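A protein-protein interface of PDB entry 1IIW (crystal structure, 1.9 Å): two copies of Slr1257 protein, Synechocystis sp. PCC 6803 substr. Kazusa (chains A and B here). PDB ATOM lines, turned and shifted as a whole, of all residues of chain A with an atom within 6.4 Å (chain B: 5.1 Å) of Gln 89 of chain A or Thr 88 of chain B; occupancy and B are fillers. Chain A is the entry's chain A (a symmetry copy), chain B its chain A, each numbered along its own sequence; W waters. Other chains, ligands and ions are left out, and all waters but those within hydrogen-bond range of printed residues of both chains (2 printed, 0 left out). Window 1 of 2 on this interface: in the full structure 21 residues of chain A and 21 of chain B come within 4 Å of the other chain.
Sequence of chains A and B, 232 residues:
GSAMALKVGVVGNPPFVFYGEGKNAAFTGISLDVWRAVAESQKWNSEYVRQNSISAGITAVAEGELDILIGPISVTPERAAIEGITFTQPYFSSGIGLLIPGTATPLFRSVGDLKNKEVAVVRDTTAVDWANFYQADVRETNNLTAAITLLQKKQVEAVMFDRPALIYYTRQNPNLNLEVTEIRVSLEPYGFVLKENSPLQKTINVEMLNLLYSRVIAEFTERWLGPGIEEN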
ATOM      1  N   VAL A  75     -28.638 -10.040  -9.405  1.00  0.00           N
ATOM      2  CA  VAL A  75     -27.630  -9.266 -10.124  1.00  0.00           C
ATOM      3  C   VAL A  75     -27.393  -7.988  -9.331  1.00  0.00           C
ATOM      4  O   VAL A  75     -28.251  -7.102  -9.306  1.00  0.00           O
ATOM      5  CB  VAL A  75     -28.106  -8.865 -11.531  1.00  0.00           C
ATOM      6  CG1 VAL A  75     -26.944  -8.269 -12.310  1.00  0.00           C
ATOM      7  CG2 VAL A  75     -28.694 -10.058 -12.260  1.00  0.00           C
ATOM      8  N   PHE A  87     -22.997 -11.812 -15.838  1.00  0.00           N
ATOM      9  CA  PHE A  87     -24.371 -12.275 -15.649  1.00  0.00           C
ATOM     10  C   PHE A  87     -25.134 -12.372 -16.962  1.00  0.00           C
ATOM     11  O   PHE A  87     -24.872 -11.612 -17.895  1.00  0.00           O
ATOM     12  CB  PHE A  87     -25.129 -11.303 -14.755  1.00  0.00           C
ATOM     13  CG  PHE A  87     -24.906 -11.522 -13.301  1.00  0.00           C
ATOM     14  CD1 PHE A  87     -23.846 -10.908 -12.650  1.00  0.00           C
ATOM     15  CD2 PHE A  87     -25.784 -12.312 -12.566  1.00  0.00           C
ATOM     16  CE1 PHE A  87     -23.659 -11.076 -11.285  1.00  0.00           C
ATOM     17  CE2 PHE A  87     -25.610 -12.490 -11.201  1.00  0.00           C
ATOM     18  CZ  PHE A  87     -24.547 -11.869 -10.553  1.00  0.00           C
ATOM     19  N   THR A  88     -26.050 -13.335 -17.055  1.00  0.00           N
ATOM     20  CA  THR A  88     -26.902 -13.444 -18.238  1.00  0.00           C
ATOM     21  C   THR A  88     -27.947 -12.339 -18.027  1.00  0.00           C
ATOM     22  O   THR A  88     -27.936 -11.647 -17.002  1.00  0.00           O
ATOM     23  CB  THR A  88     -27.726 -14.750 -18.251  1.00  0.00           C
ATOM     24  OG1 THR A  88     -28.550 -14.800 -17.077  1.00  0.00           O
ATOM     25  CG2 THR A  88     -26.849 -15.972 -18.342  1.00  0.00           C
ATOM     26  N   GLN A  89     -28.850 -12.181 -18.985  1.00  0.00           N
ATOM     27  CA  GLN A  89     -29.944 -11.230 -18.833  1.00  0.00           C
ATOM     28  C   GLN A  89     -30.810 -11.819 -17.700  1.00  0.00           C
ATOM     29  O   GLN A  89     -30.860 -13.035 -17.536  1.00  0.00           O
ATOM     30  CB  GLN A  89     -30.762 -11.168 -20.120  1.00  0.00           C
ATOM     31  CG  GLN A  89     -30.192 -10.236 -21.162  1.00  0.00           C
ATOM     32  CD  GLN A  89     -30.233  -8.805 -20.695  1.00  0.00           C
ATOM     33  OE1 GLN A  89     -31.265  -8.335 -20.236  1.00  0.00           O
ATOM     34  NE2 GLN A  89     -29.100  -8.112 -20.773  1.00  0.00           N
ATOM     35  N   PRO A  90     -31.415 -10.970 -16.853  1.00  0.00           N
ATOM     36  CA  PRO A  90     -32.252 -11.499 -15.766  1.00  0.00           C
ATOM     37  C   PRO A  90     -33.498 -12.225 -16.277  1.00  0.00           C
ATOM     38  O   PRO A  90     -33.991 -11.926 -17.369  1.00  0.00           O
ATOM     39  CB  PRO A  90     -32.596 -10.250 -14.957  1.00  0.00           C
ATOM     40  CG  PRO A  90     -32.452  -9.120 -15.965  1.00  0.00           C
ATOM     41  CD  PRO A  90     -31.229  -9.515 -16.719  1.00  0.00           C
ATOM     42  N   TYR A  91     -33.969 -13.214 -15.511  1.00  0.00           N
ATOM     43  CA  TYR A  91     -35.141 -13.997 -15.897  1.00  0.00           C
ATOM     44  C   TYR A  91     -36.290 -13.918 -14.900  1.00  0.00           C
ATOM     45  O   TYR A  91     -37.356 -14.483 -15.139  1.00  0.00           O
ATOM     46  CB  TYR A  91     -34.756 -15.471 -16.128  1.00  0.00           C
ATOM     47  CG  TYR A  91     -34.303 -16.196 -14.883  1.00  0.00           C
ATOM     48  CD1 TYR A  91     -35.197 -16.962 -14.133  1.00  0.00           C
ATOM     49  CD2 TYR A  91     -32.993 -16.065 -14.417  1.00  0.00           C
ATOM     50  CE1 TYR A  91     -34.802 -17.573 -12.943  1.00  0.00           C
ATOM     51  CE2 TYR A  91     -32.588 -16.668 -13.229  1.00  0.00           C
ATOM     52  CZ  TYR A  91     -33.495 -17.418 -12.497  1.00  0.00           C
ATOM     53  OH  TYR A  91     -33.095 -17.998 -11.316  1.00  0.00           O
ATOM     54  N   TYR A 190     -33.053 -11.767 -10.907  1.00  0.00           N
ATOM     55  CA  TYR A 190     -32.264 -12.998 -10.836  1.00  0.00           C
ATOM     56  C   TYR A 190     -31.724 -13.286 -12.219  1.00  0.00           C
ATOM     57  O   TYR A 190     -32.421 -13.094 -13.204  1.00  0.00           O
ATOM     58  CB  TYR A 190     -33.127 -14.210 -10.464  1.00  0.00           C
ATOM     59  CG  TYR A 190     -33.666 -14.261  -9.059  1.00  0.00           C
ATOM     60  CD1 TYR A 190     -34.781 -15.046  -8.757  1.00  0.00           C
ATOM     61  CD2 TYR A 190     -33.066 -13.544  -8.029  1.00  0.00           C
ATOM     62  CE1 TYR A 190     -35.283 -15.112  -7.461  1.00  0.00           C
ATOM     63  CE2 TYR A 190     -33.557 -13.602  -6.727  1.00  0.00           C
ATOM     64  CZ  TYR A 190     -34.665 -14.388  -6.452  1.00  0.00           C
ATOM     65  OH  TYR A 190     -35.150 -14.422  -5.166  1.00  0.00           O
ATOM     66  N   GLY A 191     -30.512 -13.819 -12.277  1.00  0.00           N
ATOM     67  CA  GLY A 191     -29.907 -14.190 -13.547  1.00  0.00           C
ATOM     68  C   GLY A 191     -28.999 -15.383 -13.299  1.00  0.00           C
ATOM     69  O   GLY A 191     -28.993 -15.924 -12.194  1.00  0.00           O
ATOM     70  N   PHE A 192     -28.311 -15.854 -14.330  1.00  0.00           N
ATOM     71  CA  PHE A 192     -27.363 -16.955 -14.178  1.00  0.00           C
ATOM     72  C   PHE A 192     -25.985 -16.328 -14.378  1.00  0.00           C
ATOM     73  O   PHE A 192     -25.880 -15.219 -14.884  1.00  0.00           O
ATOM     74  CB  PHE A 192     -27.591 -18.036 -15.224  1.00  0.00           C
ATOM     75  CG  PHE A 192     -28.886 -18.794 -15.070  1.00  0.00           C
ATOM     76  CD1 PHE A 192     -29.407 -19.506 -16.145  1.00  0.00           C
ATOM     77  CD2 PHE A 192     -29.556 -18.841 -13.853  1.00  0.00           C
ATOM     78  CE1 PHE A 192     -30.564 -20.251 -16.019  1.00  0.00           C
ATOM     79  CE2 PHE A 192     -30.728 -19.591 -13.716  1.00  0.00           C
ATOM     80  CZ  PHE A 192     -31.228 -20.297 -14.799  1.00  0.00           C
ATOM     81  N   ASN A 205     -28.499 -16.242 -23.599  1.00  0.00           N
ATOM     82  CA  ASN A 205     -29.303 -15.019 -23.495  1.00  0.00           C
ATOM     83  C   ASN A 205     -30.529 -15.048 -24.395  1.00  0.00           C
ATOM     84  O   ASN A 205     -31.640 -14.806 -23.934  1.00  0.00           O
ATOM     85  CB  ASN A 205     -28.458 -13.775 -23.784  1.00  0.00           C
ATOM     86  CG  ASN A 205     -27.678 -13.312 -22.567  1.00  0.00           C
ATOM     87  OD1 ASN A 205     -28.104 -13.523 -21.433  1.00  0.00           O
ATOM     88  ND2 ASN A 205     -26.534 -12.678 -22.796  1.00  0.00           N
ATOM     89  N   MET A 208     -33.099 -17.659 -23.025  1.00  0.00           N
ATOM     90  CA  MET A 208     -33.737 -17.207 -21.800  1.00  0.00           C
ATOM     91  C   MET A 208     -34.764 -16.128 -22.125  1.00  0.00           C
ATOM     92  O   MET A 208     -35.863 -16.123 -21.574  1.00  0.00           O
ATOM     93  CB  MET A 208     -32.693 -16.703 -20.807  1.00  0.00           C
ATOM     94  CG  MET A 208     -31.965 -17.832 -20.081  1.00  0.00           C
ATOM     95  SD  MET A 208     -30.624 -17.248 -19.046  1.00  0.00           S
ATOM     96  CE  MET A 208     -31.512 -16.568 -17.672  1.00  0.00           C
ATOM     97  N   LEU A 209     -34.417 -15.257 -23.065  1.00  0.00           N
ATOM     98  CA  LEU A 209     -35.308 -14.192 -23.498  1.00  0.00           C
ATOM     99  C   LEU A 209     -36.527 -14.780 -24.221  1.00  0.00           C
ATOM    100  O   LEU A 209     -37.642 -14.286 -24.047  1.00  0.00           O
ATOM    101  CB  LEU A 209     -34.554 -13.176 -24.368  1.00  0.00           C
ATOM    102  CG  LEU A 209     -33.550 -12.297 -23.603  1.00  0.00           C
ATOM    103  CD1 LEU A 209     -32.654 -11.552 -24.567  1.00  0.00           C
ATOM    104  CD2 LEU A 209     -34.290 -11.334 -22.675  1.00  0.00           C
ATOM    105  N   ILE B  68     -21.046   2.220 -28.256  1.00  0.00           N
ATOM    106  CA  ILE B  68     -22.245   1.889 -27.498  1.00  0.00           C
ATOM    107  C   ILE B  68     -23.456   2.599 -28.080  1.00  0.00           C
ATOM    108  O   ILE B  68     -23.339   3.686 -28.650  1.00  0.00           O
ATOM    109  CB  ILE B  68     -22.079   2.291 -26.001  1.00  0.00           C
ATOM    110  CG1 ILE B  68     -23.248   1.761 -25.157  1.00  0.00           C
ATOM    111  CG2 ILE B  68     -21.927   3.801 -25.868  1.00  0.00           C
ATOM    112  CD1 ILE B  68     -23.105   2.012 -23.674  1.00  0.00           C
ATOM    113  N   VAL B  75     -34.690  -5.141 -24.690  1.00  0.00           N
ATOM    114  CA  VAL B  75     -33.906  -6.367 -24.825  1.00  0.00           C
ATOM    115  C   VAL B  75     -34.861  -7.464 -25.276  1.00  0.00           C
ATOM    116  O   VAL B  75     -35.697  -7.923 -24.493  1.00  0.00           O
ATOM    117  CB  VAL B  75     -33.286  -6.804 -23.487  1.00  0.00           C
ATOM    118  CG1 VAL B  75     -32.305  -7.940 -23.729  1.00  0.00           C
ATOM    119  CG2 VAL B  75     -32.605  -5.635 -22.803  1.00  0.00           C
ATOM    120  N   THR B  86     -23.908  -7.256 -27.665  1.00  0.00           N
ATOM    121  CA  THR B  86     -24.319  -7.791 -26.383  1.00  0.00           C
ATOM    122  C   THR B  86     -24.975  -6.667 -25.584  1.00  0.00           C
ATOM    123  O   THR B  86     -24.468  -5.548 -25.548  1.00  0.00           O
ATOM    124  CB  THR B  86     -23.135  -8.390 -25.593  1.00  0.00           C
ATOM    125  OG1 THR B  86     -23.638  -9.029 -24.418  1.00  0.00           O
ATOM    126  CG2 THR B  86     -22.157  -7.317 -25.169  1.00  0.00           C
ATOM    127  N   PHE B  87     -26.146  -6.943 -25.018  1.00  0.00           N
ATOM    128  CA  PHE B  87     -26.860  -5.955 -24.212  1.00  0.00           C
ATOM    129  C   PHE B  87     -26.272  -5.813 -22.816  1.00  0.00           C
ATOM    130  O   PHE B  87     -25.735  -6.775 -22.263  1.00  0.00           O
ATOM    131  CB  PHE B  87     -28.316  -6.369 -24.050  1.00  0.00           C
ATOM    132  CG  PHE B  87     -29.183  -5.988 -25.198  1.00  0.00           C
ATOM    133  CD1 PHE B  87     -29.321  -6.834 -26.288  1.00  0.00           C
ATOM    134  CD2 PHE B  87     -29.900  -4.796 -25.173  1.00  0.00           C
ATOM    135  CE1 PHE B  87     -30.160  -6.501 -27.343  1.00  0.00           C
ATOM    136  CE2 PHE B  87     -30.742  -4.449 -26.219  1.00  0.00           C
ATOM    137  CZ  PHE B  87     -30.879  -5.304 -27.308  1.00  0.00           C
ATOM    138  N   THR B  88     -26.330  -4.605 -22.258  1.00  0.00           N
ATOM    139  CA  THR B  88     -25.882  -4.394 -20.882  1.00  0.00           C
ATOM    140  C   THR B  88     -27.044  -4.943 -20.042  1.00  0.00           C
ATOM    141  O   THR B  88     -28.065  -5.380 -20.585  1.00  0.00           O
ATOM    142  CB  THR B  88     -25.816  -2.897 -20.509  1.00  0.00           C
ATOM    143  OG1 THR B  88     -27.116  -2.312 -20.670  1.00  0.00           O
ATOM    144  CG2 THR B  88     -24.789  -2.155 -21.325  1.00  0.00           C
ATOM    145  N   GLN B  89     -26.894  -4.911 -18.724  1.00  0.00           N
ATOM    146  CA  GLN B  89     -27.979  -5.313 -17.838  1.00  0.00           C
ATOM    147  C   GLN B  89     -29.062  -4.233 -18.042  1.00  0.00           C
ATOM    148  O   GLN B  89     -28.736  -3.087 -18.338  1.00  0.00           O
ATOM    149  CB  GLN B  89     -27.502  -5.289 -16.389  1.00  0.00           C
ATOM    150  CG  GLN B  89     -26.783  -6.547 -15.961  1.00  0.00           C
ATOM    151  CD  GLN B  89     -27.709  -7.733 -15.967  1.00  0.00           C
ATOM    152  OE1 GLN B  89     -28.799  -7.669 -15.414  1.00  0.00           O
ATOM    153  NE2 GLN B  89     -27.299  -8.816 -16.624  1.00  0.00           N
ATOM    154  N   PRO B  90     -30.351  -4.605 -17.986  1.00  0.00           N
ATOM    155  CA  PRO B  90     -31.407  -3.599 -18.171  1.00  0.00           C
ATOM    156  C   PRO B  90     -31.432  -2.553 -17.055  1.00  0.00           C
ATOM    157  O   PRO B  90     -31.013  -2.833 -15.927  1.00  0.00           O
ATOM    158  CB  PRO B  90     -32.681  -4.441 -18.208  1.00  0.00           C
ATOM    159  CG  PRO B  90     -32.300  -5.702 -17.451  1.00  0.00           C
ATOM    160  CD  PRO B  90     -30.916  -5.964 -17.940  1.00  0.00           C
ATOM    161  N   GLY B 191     -32.122  -1.537 -22.148  1.00  0.00           N
ATOM    162  CA  GLY B 191     -30.707  -1.675 -21.841  1.00  0.00           C
ATOM    163  C   GLY B 191     -29.926  -0.908 -22.895  1.00  0.00           C
ATOM    164  O   GLY B 191     -30.527  -0.216 -23.716  1.00  0.00           O
ATOM    165  N   PHE B 192     -28.602  -0.943 -22.823  1.00  0.00           N
ATOM    166  CA  PHE B 192     -27.763  -0.292 -23.826  1.00  0.00           C
ATOM    167  C   PHE B 192     -27.103  -1.433 -24.598  1.00  0.00           C
ATOM    168  O   PHE B 192     -27.104  -2.568 -24.141  1.00  0.00           O
ATOM    169  CB  PHE B 192     -26.694   0.576 -23.181  1.00  0.00           C
ATOM    170  CG  PHE B 192     -27.224   1.794 -22.466  1.00  0.00           C
ATOM    171  CD1 PHE B 192     -26.437   2.439 -21.517  1.00  0.00           C
ATOM    172  CD2 PHE B 192     -28.473   2.324 -22.768  1.00  0.00           C
ATOM    173  CE1 PHE B 192     -26.876   3.586 -20.883  1.00  0.00           C
ATOM    174  CE2 PHE B 192     -28.924   3.484 -22.131  1.00  0.00           C
ATOM    175  CZ  PHE B 192     -28.123   4.114 -21.191  1.00  0.00           C
ATOM    176  N   VAL B 193     -26.548  -1.144 -25.768  1.00  0.00           N
ATOM    177  CA  VAL B 193     -25.912  -2.178 -26.578  1.00  0.00           C
ATOM    178  C   VAL B 193     -24.431  -1.888 -26.772  1.00  0.00           C
ATOM    179  O   VAL B 193     -24.034  -0.780 -27.117  1.00  0.00           O
ATOM    180  CB  VAL B 193     -26.597  -2.316 -27.953  1.00  0.00           C
ATOM    181  CG1 VAL B 193     -25.959  -3.436 -28.768  1.00  0.00           C
ATOM    182  CG2 VAL B 193     -28.089  -2.563 -27.775  1.00  0.00           C
ATOM    183  N   LEU B 194     -23.619  -2.908 -26.533  1.00  0.00           N
ATOM    184  CA  LEU B 194     -22.172  -2.826 -26.663  1.00  0.00           C
ATOM    185  C   LEU B 194     -21.714  -3.869 -27.675  1.00  0.00           C
ATOM    186  O   LEU B 194     -22.501  -4.709 -28.115  1.00  0.00           O
ATOM    187  CB  LEU B 194     -21.527  -3.142 -25.316  1.00  0.00           C
ATOM    188  CG  LEU B 194     -21.566  -2.062 -24.247  1.00  0.00           C
ATOM    189  CD1 LEU B 194     -21.441  -2.683 -22.861  1.00  0.00           C
ATOM    190  CD2 LEU B 194     -20.428  -1.086 -24.516  1.00  0.00           C
ATOM    191  N   ILE B 204     -19.332  -0.784 -17.284  1.00  0.00           N
ATOM    192  CA  ILE B 204     -20.643  -0.209 -17.573  1.00  0.00           C
ATOM    193  C   ILE B 204     -21.741  -0.915 -16.771  1.00  0.00           C
ATOM    194  O   ILE B 204     -22.568  -0.259 -16.139  1.00  0.00           O
ATOM    195  CB  ILE B 204     -20.938  -0.231 -19.095  1.00  0.00           C
ATOM    196  CG1 ILE B 204     -19.977   0.733 -19.808  1.00  0.00           C
ATOM    197  CG2 ILE B 204     -22.385   0.164 -19.367  1.00  0.00           C
ATOM    198  CD1 ILE B 204     -20.156   0.799 -21.303  1.00  0.00           C
ATOM    199  N   ASN B 205     -21.708  -2.246 -16.750  1.00  0.00           N
ATOM    200  CA  ASN B 205     -22.704  -3.015 -15.996  1.00  0.00           C
ATOM    201  C   ASN B 205     -22.701  -2.677 -14.513  1.00  0.00           C
ATOM    202  O   ASN B 205     -23.747  -2.377 -13.946  1.00  0.00           O
ATOM    203  CB  ASN B 205     -22.511  -4.520 -16.201  1.00  0.00           C
ATOM    204  CG  ASN B 205     -23.163  -5.016 -17.479  1.00  0.00           C
ATOM    205  OD1 ASN B 205     -24.152  -4.448 -17.939  1.00  0.00           O
ATOM    206  ND2 ASN B 205     -22.612  -6.076 -18.059  1.00  0.00           N
ATOM    207  N   MET B 208     -24.106   0.935 -13.988  1.00  0.00           N
ATOM    208  CA  MET B 208     -25.538   1.004 -14.226  1.00  0.00           C
ATOM    209  C   MET B 208     -26.284   0.372 -13.057  1.00  0.00           C
ATOM    210  O   MET B 208     -27.296   0.899 -12.601  1.00  0.00           O
ATOM    211  CB  MET B 208     -25.895   0.327 -15.548  1.00  0.00           C
ATOM    212  CG  MET B 208     -25.590   1.196 -16.766  1.00  0.00           C
ATOM    213  SD  MET B 208     -25.845   0.339 -18.318  1.00  0.00           S
ATOM    214  CE  MET B 208     -27.614   0.328 -18.426  1.00  0.00           C
HETATM  215  O   HOH W   1     -26.663  -9.427 -22.152  1.00  0.00           O
HETATM  216  O   HOH W   2     -24.428  -8.838 -17.775  1.00  0.00           O
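The side-chain amide oxygen (OD1) of Asn 205 of chain A sits at hydrogen-bond distance from the backbone NH (N) of Gln 89 of chain A, at 2.9 Å.
N of Gln 89 of chain B lies within hydrogen-bond range of OD1 of Asn 205 of chain B, at 2.9 Å.
The backbone carbonyl oxygen (O) of Phe 192 of chain B is in hydrogen-bond range of the backbone NH (N) of Thr 88 of chain B (2.9 Å).
The side-chain hydroxyl (OG1) of Thr 88 of chain B lies close to the side-chain sulfur (SD) of Met 208 of chain B, at 3.8 Å.
N of Thr 88 of chain A sits at hydrogen-bond distance from O of Phe 192 of chain A, at 2.9 Å.
The side-chain hydroxyl of Thr 88 of chain A lies close to the side-chain sulfur of Met 208 of chain A.
The backbone carbonyl oxygen of Thr 88 of chain A is in hydrogen-bond range of the side-chain amide nitrogen of Gln 89 of chain B (2.9 Å).
The backbone carbonyl oxygen (O) of Thr 88 of chain B sits at hydrogen-bond distance from the side-chain amide nitrogen (NE2) of Gln 89 of chain A (2.9 Å).
Among the printed residues, pairs that only touch across the chains: Gln 89 of chain A with Pro 90 of chain B (3.3 Å), Pro 90 of chain A with Gln 89 of chain B (3.3 Å), Val 75 of chain A with Gln 89 of chain B (3.7 Å), Gln 89 of chain A with Val 75 of chain B (3.7 Å), Leu 209 of chain A with Val 75 of chain B (3.7 Å), Pro 90 of chain A with Pro 90 of chain B (3.7 Å), Phe 87 of chain A with Gln 89 of chain B (3.8 Å) and Gln 89 of chain A with Phe 87 of chain B (3.8 Å).
Of the 14 printed residues of chain B, 5 touch a printed residue of chain A.
Printed residues of chain B that touch a printed residue of chain A: Val 75, Phe 87, Thr 88, Gln 89 and Pro 90.
Printed residues of chain A that touch a printed residue of chain B: Val 75, Phe 87, Thr 88, Gln 89, Pro 90 and Leu 209.
Among the printed residues, 10 pairs touch across the chains.
Among the printed residues, no Asp or Glu carboxylate lies within 4 Å of a Lys or Arg side-chain nitrogen of the other chain.
Of chain B, only Val 75 (3.7 Å), Phe 87 (3.8 Å), Thr 88 (2.9 Å) and Pro 90 (3.3 Å) come within 4 Å of Gln 89 of chain A.
Of the printed residues of chain A, Pro 90 of chain B touches Gln 89 (3.3 Å) and Pro 90 (3.7 Å).
Of the printed residues of chain B, Val 75 of chain A touches Gln 89.
Gly 191 of chain A touches none of the printed residues of chain B.
The nearest printed residue of chain A that does not touch Thr 88 of chain B is Pro 90 of chain A (6.5 Å).
The nearest printed residue of chain B that does not touch Val 75 of chain A is Asn 205 of chain B (6.9 Å).
Water W1 lies within hydrogen-bond range of O of Phe 87 of chain B (2.8 Å), NE2 of Gln 89 of chain A (3.1 Å) and ND2 of Asn 205 of chain A (3.3 Å).
Water W2 lies within hydrogen-bond range of O of Phe 87 of chain A, NE2 of Gln 89 of chain B and ND2 of Asn 205 of chain B.
Val 75 of chain A touches Gln 89 of chain B, and with the chains exchanged Gln 89 of chain A touches Val 75 of chain B.
Phe 87 of chain A touches Gln 89 of chain B, and with the chains exchanged Gln 89 of chain A touches Phe 87 of chain B.
Thr 88 of chain A touches Gln 89 of chain B, and with the chains exchanged Gln 89 of chain A touches Thr 88 of chain B.
Pro 90 of chain B touches its own counterpart, Pro 90 of chain A.
Positions printed for both chains: 75, 87, 88, 89, 90, 191, 192, 205 and 208.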
